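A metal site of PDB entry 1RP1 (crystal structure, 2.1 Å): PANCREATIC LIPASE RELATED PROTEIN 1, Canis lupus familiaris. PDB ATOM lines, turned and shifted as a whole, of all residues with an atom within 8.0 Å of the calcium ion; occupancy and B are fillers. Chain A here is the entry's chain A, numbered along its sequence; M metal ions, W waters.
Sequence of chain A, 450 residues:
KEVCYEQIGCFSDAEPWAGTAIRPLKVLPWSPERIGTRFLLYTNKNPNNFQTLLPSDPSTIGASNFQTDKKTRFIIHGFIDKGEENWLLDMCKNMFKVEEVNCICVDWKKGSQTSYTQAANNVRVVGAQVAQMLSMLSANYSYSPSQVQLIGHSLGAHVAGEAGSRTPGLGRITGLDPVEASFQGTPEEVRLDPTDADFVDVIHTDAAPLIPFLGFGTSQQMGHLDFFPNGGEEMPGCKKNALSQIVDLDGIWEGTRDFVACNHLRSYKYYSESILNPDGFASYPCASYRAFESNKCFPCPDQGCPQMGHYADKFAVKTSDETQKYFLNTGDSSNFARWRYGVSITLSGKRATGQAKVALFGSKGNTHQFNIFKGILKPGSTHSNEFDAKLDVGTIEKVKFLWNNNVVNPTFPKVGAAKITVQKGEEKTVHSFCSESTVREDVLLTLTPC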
ATOM      1  N   ALA A 157     -24.363   0.463 -14.432  1.00  0.00           N
ATOM      2  CA  ALA A 157     -24.893   0.509 -15.796  1.00  0.00           C
ATOM      3  C   ALA A 157     -24.016   1.430 -16.656  1.00  0.00           C
ATOM      4  O   ALA A 157     -23.855   1.223 -17.866  1.00  0.00           O
ATOM      5  CB  ALA A 157     -26.312   1.049 -15.802  1.00  0.00           C
ATOM      6  N   HIS A 158     -23.487   2.482 -16.040  1.00  0.00           N
ATOM      7  CA  HIS A 158     -22.630   3.410 -16.770  1.00  0.00           C
ATOM      8  C   HIS A 158     -21.193   2.866 -16.856  1.00  0.00           C
ATOM      9  O   HIS A 158     -20.480   3.164 -17.815  1.00  0.00           O
ATOM     10  CB  HIS A 158     -22.731   4.800 -16.154  1.00  0.00           C
ATOM     11  CG  HIS A 158     -24.113   5.344 -16.178  1.00  0.00           C
ATOM     12  ND1 HIS A 158     -24.837   5.499 -17.336  1.00  0.00           N
ATOM     13  CD2 HIS A 158     -24.954   5.726 -15.166  1.00  0.00           C
ATOM     14  CE1 HIS A 158     -26.053   5.949 -17.053  1.00  0.00           C
ATOM     15  NE2 HIS A 158     -26.138   6.093 -15.750  1.00  0.00           N
ATOM     16  N   ALA A 160     -20.665  -0.302 -17.345  1.00  0.00           N
ATOM     17  CA  ALA A 160     -20.884  -1.170 -18.515  1.00  0.00           C
ATOM     18  C   ALA A 160     -20.871  -0.355 -19.797  1.00  0.00           C
ATOM     19  O   ALA A 160     -20.264  -0.752 -20.792  1.00  0.00           O
ATOM     20  CB  ALA A 160     -22.227  -1.970 -18.415  1.00  0.00           C
ATOM     21  N   GLY A 161     -21.554   0.797 -19.767  1.00  0.00           N
ATOM     22  CA  GLY A 161     -21.596   1.697 -20.897  1.00  0.00           C
ATOM     23  C   GLY A 161     -20.167   2.065 -21.338  1.00  0.00           C
ATOM     24  O   GLY A 161     -19.845   1.960 -22.533  1.00  0.00           O
ATOM     25  N   GLU A 162     -19.340   2.438 -20.379  1.00  0.00           N
ATOM     26  CA  GLU A 162     -17.925   2.809 -20.636  1.00  0.00           C
ATOM     27  C   GLU A 162     -17.180   1.648 -21.287  1.00  0.00           C
ATOM     28  O   GLU A 162     -16.582   1.819 -22.340  1.00  0.00           O
ATOM     29  CB  GLU A 162     -17.212   3.199 -19.344  1.00  0.00           C
ATOM     30  CG  GLU A 162     -17.379   4.676 -18.935  1.00  0.00           C
ATOM     31  CD  GLU A 162     -16.499   5.664 -19.723  1.00  0.00           C
ATOM     32  OE1 GLU A 162     -15.856   5.267 -20.714  1.00  0.00           O
ATOM     33  OE2 GLU A 162     -16.480   6.853 -19.382  1.00  0.00           O
ATOM     34  N   ALA A 163     -17.297   0.458 -20.689  1.00  0.00           N
ATOM     35  CA  ALA A 163     -16.663  -0.745 -21.218  1.00  0.00           C
ATOM     36  C   ALA A 163     -17.074  -0.975 -22.671  1.00  0.00           C
ATOM     37  O   ALA A 163     -16.224  -1.264 -23.501  1.00  0.00           O
ATOM     38  CB  ALA A 163     -17.015  -1.979 -20.344  1.00  0.00           C
ATOM     39  N   GLY A 164     -18.380  -0.904 -22.939  1.00  0.00           N
ATOM     40  CA  GLY A 164     -18.894  -1.069 -24.283  1.00  0.00           C
ATOM     41  C   GLY A 164     -18.332  -0.011 -25.230  1.00  0.00           C
ATOM     42  O   GLY A 164     -17.916  -0.319 -26.345  1.00  0.00           O
ATOM     43  N   SER A 165     -18.348   1.240 -24.801  1.00  0.00           N
ATOM     44  CA  SER A 165     -17.799   2.328 -25.590  1.00  0.00           C
ATOM     45  C   SER A 165     -16.356   2.015 -26.041  1.00  0.00           C
ATOM     46  O   SER A 165     -15.961   2.377 -27.136  1.00  0.00           O
ATOM     47  CB  SER A 165     -17.765   3.606 -24.742  1.00  0.00           C
ATOM     48  OG  SER A 165     -17.351   4.730 -25.534  1.00  0.00           O
ATOM     49  N   ARG A 166     -15.591   1.334 -25.177  1.00  0.00           N
ATOM     50  CA  ARG A 166     -14.202   0.989 -25.425  1.00  0.00           C
ATOM     51  C   ARG A 166     -14.002  -0.376 -26.033  1.00  0.00           C
ATOM     52  O   ARG A 166     -12.874  -0.752 -26.351  1.00  0.00           O
ATOM     53  CB  ARG A 166     -13.443   1.053 -24.110  1.00  0.00           C
ATOM     54  CG  ARG A 166     -13.527   2.426 -23.439  1.00  0.00           C
ATOM     55  CD  ARG A 166     -13.066   2.367 -21.986  1.00  0.00           C
ATOM     56  NE  ARG A 166     -13.130   3.684 -21.369  1.00  0.00           N
ATOM     57  CZ  ARG A 166     -12.084   4.498 -21.237  1.00  0.00           C
ATOM     58  NH1 ARG A 166     -10.896   4.124 -21.677  1.00  0.00           N
ATOM     59  NH2 ARG A 166     -12.228   5.694 -20.694  1.00  0.00           N
ATOM     60  N   ILE A 173     -25.381  -5.404 -23.238  1.00  0.00           N
ATOM     61  CA  ILE A 173     -25.313  -4.677 -21.974  1.00  0.00           C
ATOM     62  C   ILE A 173     -26.740  -4.563 -21.463  1.00  0.00           C
ATOM     63  O   ILE A 173     -27.644  -4.145 -22.178  1.00  0.00           O
ATOM     64  CB  ILE A 173     -24.803  -3.235 -22.145  1.00  0.00           C
ATOM     65  CG1 ILE A 173     -23.259  -3.213 -22.371  1.00  0.00           C
ATOM     66  CG2 ILE A 173     -25.151  -2.411 -20.911  1.00  0.00           C
ATOM     67  CD1 ILE A 173     -22.772  -1.790 -22.749  1.00  0.00           C
ATOM     68  N   THR A 186     -25.736  14.193 -21.289  1.00  0.00           N
ATOM     69  CA  THR A 186     -24.330  14.224 -21.666  1.00  0.00           C
ATOM     70  C   THR A 186     -24.128  13.517 -23.009  1.00  0.00           C
ATOM     71  O   THR A 186     -25.060  12.917 -23.554  1.00  0.00           O
ATOM     72  CB  THR A 186     -23.470  13.500 -20.595  1.00  0.00           C
ATOM     73  OG1 THR A 186     -23.788  12.098 -20.586  1.00  0.00           O
ATOM     74  CG2 THR A 186     -23.721  14.059 -19.199  1.00  0.00           C
ATOM     75  N   PRO A 187     -22.947  13.712 -23.650  1.00  0.00           N
ATOM     76  CA  PRO A 187     -22.712  13.032 -24.918  1.00  0.00           C
ATOM     77  C   PRO A 187     -22.741  11.512 -24.601  1.00  0.00           C
ATOM     78  O   PRO A 187     -22.355  11.080 -23.506  1.00  0.00           O
ATOM     79  CB  PRO A 187     -21.308  13.489 -25.302  1.00  0.00           C
ATOM     80  CG  PRO A 187     -21.227  14.890 -24.714  1.00  0.00           C
ATOM     81  CD  PRO A 187     -21.905  14.714 -23.364  1.00  0.00           C
ATOM     82  N   GLU A 188     -23.145  10.702 -25.577  1.00  0.00           N
ATOM     83  CA  GLU A 188     -23.232   9.253 -25.405  1.00  0.00           C
ATOM     84  C   GLU A 188     -22.000   8.599 -24.786  1.00  0.00           C
ATOM     85  O   GLU A 188     -22.066   7.529 -24.169  1.00  0.00           O
ATOM     86  CB  GLU A 188     -23.610   8.568 -26.724  1.00  0.00           C
ATOM     87  CG  GLU A 188     -22.882   9.059 -27.936  1.00  0.00           C
ATOM     88  CD  GLU A 188     -23.665  10.091 -28.734  1.00  0.00           C
ATOM     89  OE1 GLU A 188     -23.701  11.267 -28.323  1.00  0.00           O
ATOM     90  OE2 GLU A 188     -24.207   9.754 -29.810  1.00  0.00           O
ATOM     91  N   GLU A 189     -20.881   9.301 -24.893  1.00  0.00           N
ATOM     92  CA  GLU A 189     -19.587   8.887 -24.369  1.00  0.00           C
ATOM     93  C   GLU A 189     -19.594   8.701 -22.838  1.00  0.00           C
ATOM     94  O   GLU A 189     -18.908   7.837 -22.283  1.00  0.00           O
ATOM     95  CB  GLU A 189     -18.577  10.003 -24.719  1.00  0.00           C
ATOM     96  CG  GLU A 189     -17.151   9.686 -24.400  1.00  0.00           C
ATOM     97  CD  GLU A 189     -16.198  10.854 -24.678  1.00  0.00           C
ATOM     98  OE1 GLU A 189     -16.637  12.016 -24.836  1.00  0.00           O
ATOM     99  OE2 GLU A 189     -14.987  10.590 -24.704  1.00  0.00           O
ATOM    100  N   VAL A 190     -20.386   9.531 -22.168  1.00  0.00           N
ATOM    101  CA  VAL A 190     -20.459   9.533 -20.723  1.00  0.00           C
ATOM    102  C   VAL A 190     -21.409   8.494 -20.093  1.00  0.00           C
ATOM    103  O   VAL A 190     -21.144   7.922 -19.037  1.00  0.00           O
ATOM    104  CB  VAL A 190     -20.862  10.962 -20.250  1.00  0.00           C
ATOM    105  CG1 VAL A 190     -20.792  11.114 -18.750  1.00  0.00           C
ATOM    106  CG2 VAL A 190     -19.966  11.992 -20.914  1.00  0.00           C
ATOM    107  N   ARG A 191     -22.466   8.163 -20.831  1.00  0.00           N
ATOM    108  CA  ARG A 191     -23.517   7.309 -20.330  1.00  0.00           C
ATOM    109  C   ARG A 191     -23.826   6.087 -21.152  1.00  0.00           C
ATOM    110  O   ARG A 191     -23.478   6.007 -22.303  1.00  0.00           O
ATOM    111  CB  ARG A 191     -24.784   8.150 -20.302  1.00  0.00           C
ATOM    112  CG  ARG A 191     -24.973   8.854 -21.653  1.00  0.00           C
ATOM    113  CD  ARG A 191     -26.274   9.628 -21.797  1.00  0.00           C
ATOM    114  NE  ARG A 191     -26.199  10.487 -22.975  1.00  0.00           N
ATOM    115  CZ  ARG A 191     -26.714  10.179 -24.159  1.00  0.00           C
ATOM    116  NH1 ARG A 191     -27.424   9.074 -24.294  1.00  0.00           N
ATOM    117  NH2 ARG A 191     -26.569  11.015 -25.181  1.00  0.00           N
ATOM    118  N   LEU A 192     -24.509   5.122 -20.556  1.00  0.00           N
ATOM    119  CA  LEU A 192     -24.917   3.911 -21.266  1.00  0.00           C
ATOM    120  C   LEU A 192     -25.954   4.400 -22.266  1.00  0.00           C
ATOM    121  O   LEU A 192     -26.782   5.217 -21.911  1.00  0.00           O
ATOM    122  CB  LEU A 192     -25.592   2.961 -20.282  1.00  0.00           C
ATOM    123  CG  LEU A 192     -26.424   1.817 -20.841  1.00  0.00           C
ATOM    124  CD1 LEU A 192     -25.513   0.880 -21.644  1.00  0.00           C
ATOM    125  CD2 LEU A 192     -27.060   1.078 -19.670  1.00  0.00           C
ATOM    126  N   ASP A 193     -25.871   3.913 -23.505  1.00  0.00           N
ATOM    127  CA  ASP A 193     -26.788   4.294 -24.591  1.00  0.00           C
ATOM    128  C   ASP A 193     -26.696   3.131 -25.577  1.00  0.00           C
ATOM    129  O   ASP A 193     -25.784   2.308 -25.459  1.00  0.00           O
ATOM    130  CB  ASP A 193     -26.371   5.635 -25.223  1.00  0.00           C
ATOM    131  CG  ASP A 193     -25.112   5.538 -26.068  1.00  0.00           C
ATOM    132  OD1 ASP A 193     -23.996   5.558 -25.520  1.00  0.00           O
ATOM    133  OD2 ASP A 193     -25.247   5.477 -27.290  1.00  0.00           O
ATOM    134  N   PRO A 194     -27.594   3.050 -26.571  1.00  0.00           N
ATOM    135  CA  PRO A 194     -27.574   1.944 -27.536  1.00  0.00           C
ATOM    136  C   PRO A 194     -26.264   1.655 -28.300  1.00  0.00           C
ATOM    137  O   PRO A 194     -26.006   0.488 -28.641  1.00  0.00           O
ATOM    138  CB  PRO A 194     -28.715   2.293 -28.500  1.00  0.00           C
ATOM    139  CG  PRO A 194     -29.632   3.110 -27.632  1.00  0.00           C
ATOM    140  CD  PRO A 194     -28.639   4.012 -26.948  1.00  0.00           C
ATOM    141  N   THR A 195     -25.441   2.687 -28.529  1.00  0.00           N
ATOM    142  CA  THR A 195     -24.172   2.522 -29.274  1.00  0.00           C
ATOM    143  C   THR A 195     -23.088   1.771 -28.522  1.00  0.00           C
ATOM    144  O   THR A 195     -22.056   1.408 -29.105  1.00  0.00           O
ATOM    145  CB  THR A 195     -23.571   3.865 -29.761  1.00  0.00           C
ATOM    146  OG1 THR A 195     -23.329   4.742 -28.657  1.00  0.00           O
ATOM    147  CG2 THR A 195     -24.514   4.523 -30.733  1.00  0.00           C
ATOM    148  N   ASP A 196     -23.318   1.512 -27.236  1.00  0.00           N
ATOM    149  CA  ASP A 196     -22.335   0.807 -26.429  1.00  0.00           C
ATOM    150  C   ASP A 196     -22.257  -0.666 -26.665  1.00  0.00           C
ATOM    151  O   ASP A 196     -21.331  -1.299 -26.191  1.00  0.00           O
ATOM    152  CB  ASP A 196     -22.615   1.043 -24.938  1.00  0.00           C
ATOM    153  CG  ASP A 196     -22.364   2.467 -24.507  1.00  0.00           C
ATOM    154  OD1 ASP A 196     -21.438   3.090 -25.054  1.00  0.00           O
ATOM    155  OD2 ASP A 196     -23.080   2.959 -23.611  1.00  0.00           O
ATOM    156  N   ALA A 197     -23.269  -1.257 -27.296  1.00  0.00           N
ATOM    157  CA  ALA A 197     -23.251  -2.711 -27.542  1.00  0.00           C
ATOM    158  C   ALA A 197     -24.209  -3.046 -28.646  1.00  0.00           C
ATOM    159  O   ALA A 197     -25.006  -2.199 -29.000  1.00  0.00           O
ATOM    160  CB  ALA A 197     -23.631  -3.473 -26.295  1.00  0.00           C
ATOM    161  N   MET A 222     -32.923   4.471 -22.778  1.00  0.00           N
ATOM    162  CA  MET A 222     -31.479   4.345 -22.938  1.00  0.00           C
ATOM    163  C   MET A 222     -31.001   3.145 -23.753  1.00  0.00           C
ATOM    164  O   MET A 222     -29.783   2.991 -23.941  1.00  0.00           O
ATOM    165  CB  MET A 222     -30.809   4.304 -21.571  1.00  0.00           C
ATOM    166  CG  MET A 222     -31.231   5.390 -20.603  1.00  0.00           C
ATOM    167  SD  MET A 222     -30.519   5.116 -19.013  1.00  0.00           S
ATOM    168  CE  MET A 222     -28.800   5.430 -19.371  1.00  0.00           C
HETATM  169 CA    CA M   1     -22.162   5.297 -24.044  1.00  0.00          CA
HETATM  170  O   HOH W   1     -20.428   5.409 -22.595  1.00  0.00           O
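Four residues have an atom within 4 Å of the calcium ion: Glu 188, Arg 191, Asp 193 and Asp 196. The nearest printed residue that does not touch the calcium ion is Leu 192 (4.2 Å).
NE of Arg 191 sits at hydrogen-bond distance from O of Thr 186 (2.7 Å). The side-chain hydroxyl of Thr 195 sits at hydrogen-bond distance from the side-chain carboxylate of Asp 193 (2.5 Å).
Water W1 bridges O of Glu 189 and O of Gly 161.
The calcium ion is bound by the backbone carbonyl oxygen (O) of Glu 188 (2.2 Å). The calcium ion is bound by water W1, 2.3 Å away. O of Arg 191 is bound to the calcium ion (2.3 Å). The side-chain carboxylate (OD1) of Asp 193 binds the calcium ion (2.4 Å). The calcium ion is bound by OD1 of Asp 196, 2.5 Å away. The calcium ion is bound by OD2 of Asp 196, at 2.5 Å. The calcium ion has six donor atoms within binding distance.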
